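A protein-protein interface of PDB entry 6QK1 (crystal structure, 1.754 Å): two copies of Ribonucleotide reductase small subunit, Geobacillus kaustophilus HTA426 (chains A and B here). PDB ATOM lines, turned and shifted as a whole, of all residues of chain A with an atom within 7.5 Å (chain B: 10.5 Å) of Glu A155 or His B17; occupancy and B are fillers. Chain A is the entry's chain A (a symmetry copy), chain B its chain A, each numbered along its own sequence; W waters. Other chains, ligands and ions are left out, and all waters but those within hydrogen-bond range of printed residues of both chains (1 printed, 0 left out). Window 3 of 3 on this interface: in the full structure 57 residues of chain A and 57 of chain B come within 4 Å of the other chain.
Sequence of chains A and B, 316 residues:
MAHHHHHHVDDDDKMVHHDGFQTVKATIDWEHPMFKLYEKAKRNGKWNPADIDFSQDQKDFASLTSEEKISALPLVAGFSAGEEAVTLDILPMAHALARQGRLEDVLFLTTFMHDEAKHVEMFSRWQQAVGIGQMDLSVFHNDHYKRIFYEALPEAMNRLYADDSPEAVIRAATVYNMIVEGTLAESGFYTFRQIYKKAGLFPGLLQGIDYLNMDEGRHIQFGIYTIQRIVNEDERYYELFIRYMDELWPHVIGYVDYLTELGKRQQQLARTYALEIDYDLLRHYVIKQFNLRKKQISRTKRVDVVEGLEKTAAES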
ATOM      1  N   ASP A  89       1.675   6.266  21.771  1.00  0.00           N
ATOM      2  CA  ASP A  89       0.305   6.174  21.276  1.00  0.00           C
ATOM      3  C   ASP A  89      -0.663   5.466  22.227  1.00  0.00           C
ATOM      4  O   ASP A  89      -1.864   5.382  21.935  1.00  0.00           O
ATOM      5  CB  ASP A  89       0.324   5.494  19.908  1.00  0.00           C
ATOM      6  CG  ASP A  89       0.988   6.347  18.844  1.00  0.00           C
ATOM      7  OD1 ASP A  89       1.177   7.564  19.101  1.00  0.00           O
ATOM      8  OD2 ASP A  89       1.356   5.803  17.768  1.00  0.00           O
ATOM      9  N   LYS A 146       5.218   1.458   7.494  1.00  0.00           N
ATOM     10  CA  LYS A 146       4.843   2.844   7.740  1.00  0.00           C
ATOM     11  C   LYS A 146       3.336   3.006   7.842  1.00  0.00           C
ATOM     12  O   LYS A 146       2.836   3.754   8.689  1.00  0.00           O
ATOM     13  CB  LYS A 146       5.395   3.720   6.616  1.00  0.00           C
ATOM     14  CG  LYS A 146       6.880   3.886   6.695  1.00  0.00           C
ATOM     15  CD  LYS A 146       7.415   4.805   5.607  1.00  0.00           C
ATOM     16  CE  LYS A 146       8.922   4.984   5.777  1.00  0.00           C
ATOM     17  NZ  LYS A 146       9.524   5.961   4.838  1.00  0.00           N
ATOM     18  N   ARG A 147       2.594   2.335   6.971  1.00  0.00           N
ATOM     19  CA  ARG A 147       1.148   2.461   7.020  1.00  0.00           C
ATOM     20  C   ARG A 147       0.613   2.007   8.370  1.00  0.00           C
ATOM     21  O   ARG A 147      -0.355   2.586   8.884  1.00  0.00           O
ATOM     22  CB  ARG A 147       0.494   1.669   5.889  1.00  0.00           C
ATOM     23  CG  ARG A 147      -1.038   1.625   5.986  1.00  0.00           C
ATOM     24  CD  ARG A 147      -1.692   3.057   6.011  1.00  0.00           C
ATOM     25  NE  ARG A 147      -3.032   3.069   6.619  1.00  0.00           N
ATOM     26  CZ  ARG A 147      -3.655   4.160   7.087  1.00  0.00           C
ATOM     27  NH1 ARG A 147      -3.074   5.360   7.026  1.00  0.00           N
ATOM     28  NH2 ARG A 147      -4.870   4.054   7.628  1.00  0.00           N
ATOM     29  N   ILE A 148       1.216   0.971   8.963  1.00  0.00           N
ATOM     30  CA  ILE A 148       0.774   0.522  10.272  1.00  0.00           C
ATOM     31  C   ILE A 148       1.265   1.471  11.356  1.00  0.00           C
ATOM     32  O   ILE A 148       0.476   2.014  12.142  1.00  0.00           O
ATOM     33  CB  ILE A 148       1.236  -0.929  10.526  1.00  0.00           C
ATOM     34  CG1 ILE A 148       0.592  -1.833   9.467  1.00  0.00           C
ATOM     35  CG2 ILE A 148       0.890  -1.390  11.965  1.00  0.00           C
ATOM     36  CD1 ILE A 148       0.868  -3.334   9.633  1.00  0.00           C
ATOM     37  N   PHE A 149       2.572   1.694  11.412  1.00  0.00           N
ATOM     38  CA  PHE A 149       3.160   2.326  12.591  1.00  0.00           C
ATOM     39  C   PHE A 149       3.265   3.839  12.496  1.00  0.00           C
ATOM     40  O   PHE A 149       3.166   4.519  13.529  1.00  0.00           O
ATOM     41  CB  PHE A 149       4.540   1.743  12.844  1.00  0.00           C
ATOM     42  CG  PHE A 149       4.498   0.360  13.430  1.00  0.00           C
ATOM     43  CD1 PHE A 149       4.331   0.172  14.795  1.00  0.00           C
ATOM     44  CD2 PHE A 149       4.605  -0.753  12.604  1.00  0.00           C
ATOM     45  CE1 PHE A 149       4.282  -1.108  15.327  1.00  0.00           C
ATOM     46  CE2 PHE A 149       4.568  -2.020  13.139  1.00  0.00           C
ATOM     47  CZ  PHE A 149       4.403  -2.194  14.501  1.00  0.00           C
ATOM     48  N   TYR A 150       3.548   4.381  11.301  1.00  0.00           N
ATOM     49  CA  TYR A 150       3.625   5.840  11.184  1.00  0.00           C
ATOM     50  C   TYR A 150       2.251   6.473  11.021  1.00  0.00           C
ATOM     51  O   TYR A 150       2.097   7.664  11.316  1.00  0.00           O
ATOM     52  CB  TYR A 150       4.499   6.279  10.008  1.00  0.00           C
ATOM     53  CG  TYR A 150       5.996   5.975  10.052  1.00  0.00           C
ATOM     54  CD1 TYR A 150       6.932   6.941   9.617  1.00  0.00           C
ATOM     55  CD2 TYR A 150       6.479   4.752  10.464  1.00  0.00           C
ATOM     56  CE1 TYR A 150       8.301   6.681   9.602  1.00  0.00           C
ATOM     57  CE2 TYR A 150       7.853   4.479  10.475  1.00  0.00           C
ATOM     58  CZ  TYR A 150       8.766   5.453  10.037  1.00  0.00           C
ATOM     59  OH  TYR A 150      10.134   5.203  10.029  1.00  0.00           O
ATOM     60  N   GLU A 151       1.242   5.704  10.608  1.00  0.00           N
ATOM     61  CA  GLU A 151      -0.069   6.276  10.288  1.00  0.00           C
ATOM     62  C   GLU A 151      -1.267   5.653  11.001  1.00  0.00           C
ATOM     63  O   GLU A 151      -1.950   6.320  11.790  1.00  0.00           O
ATOM     64  CB  GLU A 151      -0.296   6.185   8.771  1.00  0.00           C
ATOM     65  CG  GLU A 151       0.804   6.886   7.972  1.00  0.00           C
ATOM     66  CD  GLU A 151       0.662   6.719   6.465  1.00  0.00           C
ATOM     67  OE1 GLU A 151       1.567   7.187   5.735  1.00  0.00           O
ATOM     68  OE2 GLU A 151      -0.340   6.120   6.018  1.00  0.00           O
ATOM     69  N   ALA A 152      -1.573   4.385  10.710  1.00  0.00           N
ATOM     70  CA  ALA A 152      -2.838   3.797  11.163  1.00  0.00           C
ATOM     71  C   ALA A 152      -2.923   3.713  12.686  1.00  0.00           C
ATOM     72  O   ALA A 152      -4.009   3.865  13.267  1.00  0.00           O
ATOM     73  CB  ALA A 152      -3.017   2.395  10.567  1.00  0.00           C
ATOM     74  N   LEU A 153      -1.800   3.376  13.336  1.00  0.00           N
ATOM     75  CA  LEU A 153      -1.784   3.289  14.796  1.00  0.00           C
ATOM     76  C   LEU A 153      -2.023   4.657  15.417  1.00  0.00           C
ATOM     77  O   LEU A 153      -2.954   4.798  16.218  1.00  0.00           O
ATOM     78  CB  LEU A 153      -0.467   2.659  15.266  1.00  0.00           C
ATOM     79  CG  LEU A 153      -0.179   2.610  16.756  1.00  0.00           C
ATOM     80  CD1 LEU A 153      -1.197   1.682  17.439  1.00  0.00           C
ATOM     81  CD2 LEU A 153       1.224   2.147  17.031  1.00  0.00           C
ATOM     82  N   PRO A 154      -1.235   5.691  15.115  1.00  0.00           N
ATOM     83  CA  PRO A 154      -1.525   6.985  15.730  1.00  0.00           C
ATOM     84  C   PRO A 154      -2.892   7.527  15.357  1.00  0.00           C
ATOM     85  O   PRO A 154      -3.521   8.200  16.189  1.00  0.00           O
ATOM     86  CB  PRO A 154      -0.374   7.886  15.231  1.00  0.00           C
ATOM     87  CG  PRO A 154       0.281   7.115  14.114  1.00  0.00           C
ATOM     88  CD  PRO A 154       0.075   5.686  14.433  1.00  0.00           C
ATOM     89  N   GLU A 155      -3.387   7.258  14.143  1.00  0.00           N
ATOM     90  CA  GLU A 155      -4.717   7.749  13.765  1.00  0.00           C
ATOM     91  C   GLU A 155      -5.795   7.154  14.657  1.00  0.00           C
ATOM     92  O   GLU A 155      -6.657   7.873  15.195  1.00  0.00           O
ATOM     93  CB  GLU A 155      -5.024   7.414  12.296  1.00  0.00           C
ATOM     94  CG  GLU A 155      -4.402   8.312  11.311  1.00  0.00           C
ATOM     95  CD  GLU A 155      -4.673   7.894   9.861  1.00  0.00           C
ATOM     96  OE1 GLU A 155      -5.408   6.922   9.638  1.00  0.00           O
ATOM     97  OE2 GLU A 155      -4.123   8.535   8.947  1.00  0.00           O
ATOM     98  N   ALA A 156      -5.749   5.827  14.845  1.00  0.00           N
ATOM     99  CA  ALA A 156      -6.766   5.139  15.626  1.00  0.00           C
ATOM    100  C   ALA A 156      -6.730   5.543  17.095  1.00  0.00           C
ATOM    101  O   ALA A 156      -7.771   5.642  17.752  1.00  0.00           O
ATOM    102  CB  ALA A 156      -6.594   3.625  15.506  1.00  0.00           C
ATOM    103  N   MET A 157      -5.543   5.717  17.648  1.00  0.00           N
ATOM    104  CA  MET A 157      -5.438   6.078  19.063  1.00  0.00           C
ATOM    105  C   MET A 157      -5.816   7.544  19.288  1.00  0.00           C
ATOM    106  O   MET A 157      -6.605   7.870  20.200  1.00  0.00           O
ATOM    107  CB  MET A 157      -4.006   5.812  19.585  1.00  0.00           C
ATOM    108  CG  MET A 157      -3.477   4.351  19.333  1.00  0.00           C
ATOM    109  SD  MET A 157      -4.584   3.039  19.781  1.00  0.00           S
ATOM    110  CE  MET A 157      -4.659   3.285  21.481  1.00  0.00           C
ATOM    111  N   ASN A 158      -5.267   8.445  18.483  1.00  0.00           N
ATOM    112  CA  ASN A 158      -5.554   9.863  18.690  1.00  0.00           C
ATOM    113  C   ASN A 158      -7.016  10.194  18.487  1.00  0.00           C
ATOM    114  O   ASN A 158      -7.494  11.164  19.084  1.00  0.00           O
ATOM    115  CB  ASN A 158      -4.735  10.756  17.780  1.00  0.00           C
ATOM    116  CG  ASN A 158      -3.495  11.190  18.444  1.00  0.00           C
ATOM    117  OD1 ASN A 158      -3.479  12.221  19.109  1.00  0.00           O
ATOM    118  ND2 ASN A 158      -2.446  10.387  18.329  1.00  0.00           N
ATOM    119  N   ARG A 159      -7.727   9.435  17.638  1.00  0.00           N
ATOM    120  CA  ARG A 159      -9.183   9.601  17.504  1.00  0.00           C
ATOM    121  C   ARG A 159      -9.895   9.612  18.849  1.00  0.00           C
ATOM    122  O   ARG A 159     -10.917  10.294  19.016  1.00  0.00           O
ATOM    123  CB  ARG A 159      -9.737   8.467  16.610  1.00  0.00           C
ATOM    124  CG  ARG A 159     -11.282   8.332  16.632  1.00  0.00           C
ATOM    125  CD  ARG A 159     -11.741   7.203  15.658  1.00  0.00           C
ATOM    126  NE  ARG A 159     -13.196   7.060  15.651  1.00  0.00           N
ATOM    127  CZ  ARG A 159     -13.838   6.078  15.026  1.00  0.00           C
ATOM    128  NH1 ARG A 159     -13.152   5.140  14.361  1.00  0.00           N
ATOM    129  NH2 ARG A 159     -15.171   6.029  15.075  1.00  0.00           N
ATOM    130  N   LEU A 160      -9.376   8.875  19.837  1.00  0.00           N
ATOM    131  CA  LEU A 160     -10.060   8.708  21.111  1.00  0.00           C
ATOM    132  C   LEU A 160     -10.191  10.007  21.886  1.00  0.00           C
ATOM    133  O   LEU A 160     -11.052  10.086  22.766  1.00  0.00           O
ATOM    134  CB  LEU A 160      -9.340   7.694  21.987  1.00  0.00           C
ATOM    135  CG  LEU A 160      -9.314   6.252  21.416  1.00  0.00           C
ATOM    136  CD1 LEU A 160      -8.561   5.285  22.407  1.00  0.00           C
ATOM    137  CD2 LEU A 160     -10.741   5.725  21.163  1.00  0.00           C
ATOM    138  N   ARG A 171     -11.748  -0.137  17.615  1.00  0.00           N
ATOM    139  CA  ARG A 171     -10.772  -0.042  16.557  1.00  0.00           C
ATOM    140  C   ARG A 171      -9.380   0.208  17.120  1.00  0.00           C
ATOM    141  O   ARG A 171      -8.396  -0.353  16.622  1.00  0.00           O
ATOM    142  CB  ARG A 171     -11.100   1.049  15.557  1.00  0.00           C
ATOM    143  CG  ARG A 171     -10.337   0.719  14.327  1.00  0.00           C
ATOM    144  CD  ARG A 171     -10.196   1.784  13.423  1.00  0.00           C
ATOM    145  NE  ARG A 171      -9.730   1.287  12.140  1.00  0.00           N
ATOM    146  CZ  ARG A 171      -9.816   2.018  11.041  1.00  0.00           C
ATOM    147  NH1 ARG A 171     -10.306   3.249  11.128  1.00  0.00           N
ATOM    148  NH2 ARG A 171      -9.407   1.550   9.876  1.00  0.00           N
ATOM    149  N   ALA A 172      -9.289   1.065  18.136  1.00  0.00           N
ATOM    150  CA  ALA A 172      -7.997   1.367  18.757  1.00  0.00           C
ATOM    151  C   ALA A 172      -7.361   0.118  19.375  1.00  0.00           C
ATOM    152  O   ALA A 172      -6.184  -0.148  19.164  1.00  0.00           O
ATOM    153  CB  ALA A 172      -8.214   2.452  19.801  1.00  0.00           C
ATOM    154  N   VAL A 175      -6.172  -2.372  16.522  1.00  0.00           N
ATOM    155  CA  VAL A 175      -4.909  -2.017  15.872  1.00  0.00           C
ATOM    156  C   VAL A 175      -3.753  -2.171  16.844  1.00  0.00           C
ATOM    157  O   VAL A 175      -2.673  -2.666  16.478  1.00  0.00           O
ATOM    158  CB  VAL A 175      -4.956  -0.573  15.307  1.00  0.00           C
ATOM    159  CG1 VAL A 175      -3.621  -0.189  14.686  1.00  0.00           C
ATOM    160  CG2 VAL A 175      -6.039  -0.395  14.234  1.00  0.00           C
ATOM    161  N   VAL B  16      -2.436  11.926  14.349  1.00  0.00           N
ATOM    162  CA  VAL B  16      -1.532  12.549  13.390  1.00  0.00           C
ATOM    163  C   VAL B  16      -0.192  11.778  13.332  1.00  0.00           C
ATOM    164  O   VAL B  16       0.387  11.381  14.342  1.00  0.00           O
ATOM    165  CB  VAL B  16      -1.325  14.072  13.712  1.00  0.00           C
ATOM    166  CG1 VAL B  16      -0.365  14.297  14.887  1.00  0.00           C
ATOM    167  CG2 VAL B  16      -0.863  14.849  12.478  1.00  0.00           C
ATOM    168  N   HIS B  17       0.295  11.618  12.110  1.00  0.00           N
ATOM    169  CA  HIS B  17       1.356  10.668  11.790  1.00  0.00           C
ATOM    170  C   HIS B  17       2.632  10.906  12.608  1.00  0.00           C
ATOM    171  O   HIS B  17       2.938  12.029  13.015  1.00  0.00           O
ATOM    172  CB  HIS B  17       1.672  10.765  10.287  1.00  0.00           C
ATOM    173  CG  HIS B  17       0.504  10.446   9.385  1.00  0.00           C
ATOM    174  ND1 HIS B  17      -0.742  10.080   9.862  1.00  0.00           N
ATOM    175  CD2 HIS B  17       0.403  10.438   8.030  1.00  0.00           C
ATOM    176  CE1 HIS B  17      -1.556   9.863   8.842  1.00  0.00           C
ATOM    177  NE2 HIS B  17      -0.887  10.070   7.720  1.00  0.00           N
ATOM    178  N   HIS B  18       3.396   9.831  12.831  1.00  0.00           N
ATOM    179  CA  HIS B  18       4.786   9.963  13.264  1.00  0.00           C
ATOM    180  C   HIS B  18       5.678  10.244  12.047  1.00  0.00           C
ATOM    181  O   HIS B  18       5.548   9.586  11.020  1.00  0.00           O
ATOM    182  CB  HIS B  18       5.262   8.685  13.973  1.00  0.00           C
ATOM    183  CG  HIS B  18       4.481   8.327  15.198  1.00  0.00           C
ATOM    184  ND1 HIS B  18       4.551   9.057  16.369  1.00  0.00           N
ATOM    185  CD2 HIS B  18       3.636   7.294  15.450  1.00  0.00           C
ATOM    186  CE1 HIS B  18       3.762   8.504  17.278  1.00  0.00           C
ATOM    187  NE2 HIS B  18       3.200   7.430  16.749  1.00  0.00           N
ATOM    188  N   ASP B  19       6.573  11.229  12.145  1.00  0.00           N
ATOM    189  CA  ASP B  19       7.499  11.483  11.037  1.00  0.00           C
ATOM    190  C   ASP B  19       8.758  10.618  11.118  1.00  0.00           C
ATOM    191  O   ASP B  19       9.467  10.480  10.117  1.00  0.00           O
ATOM    192  CB  ASP B  19       7.875  12.979  10.971  1.00  0.00           C
ATOM    193  CG  ASP B  19       6.750  13.865  10.353  1.00  0.00           C
ATOM    194  OD1 ASP B  19       5.969  13.377   9.501  1.00  0.00           O
ATOM    195  OD2 ASP B  19       6.648  15.062  10.713  1.00  0.00           O
ATOM    196  N   GLY B  20       9.029  10.020  12.268  1.00  0.00           N
ATOM    197  CA  GLY B  20      10.150   9.115  12.449  1.00  0.00           C
ATOM    198  C   GLY B  20      10.277   8.839  13.932  1.00  0.00           C
ATOM    199  O   GLY B  20       9.524   9.379  14.742  1.00  0.00           O
ATOM    200  N   PHE B  21      11.265   8.014  14.285  1.00  0.00           N
ATOM    201  CA  PHE B  21      11.445   7.604  15.667  1.00  0.00           C
ATOM    202  C   PHE B  21      12.894   7.801  16.089  1.00  0.00           C
ATOM    203  O   PHE B  21      13.823   7.347  15.405  1.00  0.00           O
ATOM    204  CB  PHE B  21      10.995   6.151  15.834  1.00  0.00           C
ATOM    205  CG  PHE B  21       9.553   5.956  15.487  1.00  0.00           C
ATOM    206  CD1 PHE B  21       8.577   6.270  16.420  1.00  0.00           C
ATOM    207  CD2 PHE B  21       9.156   5.495  14.232  1.00  0.00           C
ATOM    208  CE1 PHE B  21       7.227   6.144  16.120  1.00  0.00           C
ATOM    209  CE2 PHE B  21       7.792   5.352  13.925  1.00  0.00           C
ATOM    210  CZ  PHE B  21       6.835   5.672  14.869  1.00  0.00           C
ATOM    211  N   HIS B  95       1.108  13.663  27.160  1.00  0.00           N
ATOM    212  CA  HIS B  95       0.762  13.866  25.756  1.00  0.00           C
ATOM    213  C   HIS B  95       1.501  15.064  25.146  1.00  0.00           C
ATOM    214  O   HIS B  95       2.107  14.965  24.065  1.00  0.00           O
ATOM    215  CB  HIS B  95      -0.741  14.080  25.622  1.00  0.00           C
ATOM    216  CG  HIS B  95      -1.160  14.493  24.240  1.00  0.00           C
ATOM    217  ND1 HIS B  95      -1.282  13.597  23.201  1.00  0.00           N
ATOM    218  CD2 HIS B  95      -1.433  15.717  23.721  1.00  0.00           C
ATOM    219  CE1 HIS B  95      -1.650  14.246  22.109  1.00  0.00           C
ATOM    220  NE2 HIS B  95      -1.751  15.530  22.399  1.00  0.00           N
ATOM    221  N   ALA B  98       5.122  14.409  24.725  1.00  0.00           N
ATOM    222  CA  ALA B  98       5.277  13.413  23.663  1.00  0.00           C
ATOM    223  C   ALA B  98       5.201  14.054  22.275  1.00  0.00           C
ATOM    224  O   ALA B  98       6.022  13.781  21.400  1.00  0.00           O
ATOM    225  CB  ALA B  98       4.191  12.351  23.819  1.00  0.00           C
ATOM    226  N   ARG B  99       4.213  14.920  22.070  1.00  0.00           N
ATOM    227  CA  ARG B  99       3.988  15.570  20.781  1.00  0.00           C
ATOM    228  C   ARG B  99       5.094  16.559  20.472  1.00  0.00           C
ATOM    229  O   ARG B  99       5.338  16.882  19.296  1.00  0.00           O
ATOM    230  CB  ARG B  99       2.588  16.231  20.844  1.00  0.00           C
ATOM    231  CG  ARG B  99       1.814  16.538  19.558  1.00  0.00           C
ATOM    232  CD  ARG B  99       0.382  17.104  19.876  1.00  0.00           C
ATOM    233  NE  ARG B  99       0.332  18.003  21.046  1.00  0.00           N
ATOM    234  CZ  ARG B  99      -0.788  18.453  21.642  1.00  0.00           C
ATOM    235  NH1 ARG B  99      -2.002  18.104  21.192  1.00  0.00           N
ATOM    236  NH2 ARG B  99      -0.696  19.263  22.712  1.00  0.00           N
ATOM    237  N   GLN B 100       5.781  17.049  21.499  1.00  0.00           N
ATOM    238  CA  GLN B 100       6.976  17.848  21.281  1.00  0.00           C
ATOM    239  C   GLN B 100       8.224  17.017  21.054  1.00  0.00           C
ATOM    240  O   GLN B 100       9.304  17.599  20.893  1.00  0.00           O
ATOM    241  CB  GLN B 100       7.180  18.796  22.466  1.00  0.00           C
ATOM    242  CG  GLN B 100       6.058  19.821  22.674  1.00  0.00           C
ATOM    243  CD  GLN B 100       6.283  20.784  23.810  1.00  0.00           C
ATOM    244  OE1 GLN B 100       7.279  20.714  24.527  1.00  0.00           O
ATOM    245  NE2 GLN B 100       5.370  21.737  23.944  1.00  0.00           N
ATOM    246  N   GLY B 101       8.140  15.685  21.051  1.00  0.00           N
ATOM    247  CA  GLY B 101       9.318  14.878  20.809  1.00  0.00           C
ATOM    248  C   GLY B 101      10.261  14.725  21.981  1.00  0.00           C
ATOM    249  O   GLY B 101      11.398  14.278  21.794  1.00  0.00           O
HETATM  250  O   HOH W   1      12.192   6.560  11.898  1.00  0.00           O
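Printed residues of chain A that touch a printed residue of chain B: Asp A89, Phe A149, Tyr A150, Glu A151, Pro A154 and Glu A155.
Hydrophobic or aromatic side chains of chain A that line the printed part of chain B: Tyr A150 and Pro A154.
Printed residues of chain B that touch a printed residue of chain A: Val B16, His B17, His B18 and Phe B21.
Hydrophobic or aromatic side chains of chain B within 4 Å of the printed part of chain A: His B17, His B18 and Phe B21.
No position is printed for both chains.
Phe A149 touches His B18.
O of Tyr A150 touches CA of His B17, 3.1 Å away.
CE2 of Phe B21 touches CE2 of Tyr A150 (3.6 Å).
Glu A151 touches His B17 (CG to CD2, 3.6 Å).
Pro A154 touches Val B16 (CB to O, 3.7 Å).
Pro A154 touches His B18 (CG to CD2, 3.6 Å).
Glu A155 touches His B17 (OE2 to CE1, 2.9 Å).
The side-chain carboxylate (OD2) of Asp A89 is in hydrogen-bond range of a ring nitrogen (NE2) of His B18, at 2.7 Å.
N of His B18 sits at hydrogen-bond distance from O of Tyr A150 (2.9 Å).
Water W1 lies within hydrogen-bond range of N of Phe B21 and OH of Tyr A150.
The backbone NH of Glu A151 lies within hydrogen-bond range of the backbone carbonyl oxygen of Lys A146.
The guanidinium group (NH1) of Arg A147 is in salt-bridge range of the side-chain carboxylate (OE2) of Glu A151 (3.0 Å).
The guanidinium group (NH2) of Arg A147 is in salt-bridge range of the side-chain carboxylate (OE1) of Glu A155 (3.5 Å).
O of Pro A154 lies within hydrogen-bond range of ND2 of Asn A158 (3.2 Å).
Printed residues of chain B within 4 Å of Asp A89: His B18 (2.7 Å).
Printed residues of chain B within 4 Å of Phe A149: His B18 (3.4 Å).
Of the printed residues of chain B, Tyr A150 touches His B17 (3.1 Å), His B18 (2.9 Å) and Phe B21 (3.6 Å).
Of the printed residues of chain B, Glu A151 touches His B17.
No residue of chain B comes within 4 Å of Ala A152.
Pro A154 touches just these residues of chain B: Val B16 (3.7 Å) and His B18 (3.6 Å).
Of chain B, only His B17 (2.9 Å) comes within 4 Å of Glu A155.
No residue of chain B comes within 4 Å of Ala A156.
Of the printed residues of chain A, Val B16 touches Pro A154.
Of chain A, only Tyr A150, Glu A151 and Glu A155 come within 4 Å of His B17.
Of the printed residues of chain A, His B18 touches Asp A89 (2.7 Å), Phe A149 (3.4 Å), Tyr A150 (2.9 Å) and Pro A154 (3.6 Å).
Asp B19 touches none of the printed residues of chain A.
Arg B99 touches none of the printed residues of chain A.
The nearest residue of chain B that does not touch Glu A155 is Val B16 (4.8 Å).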
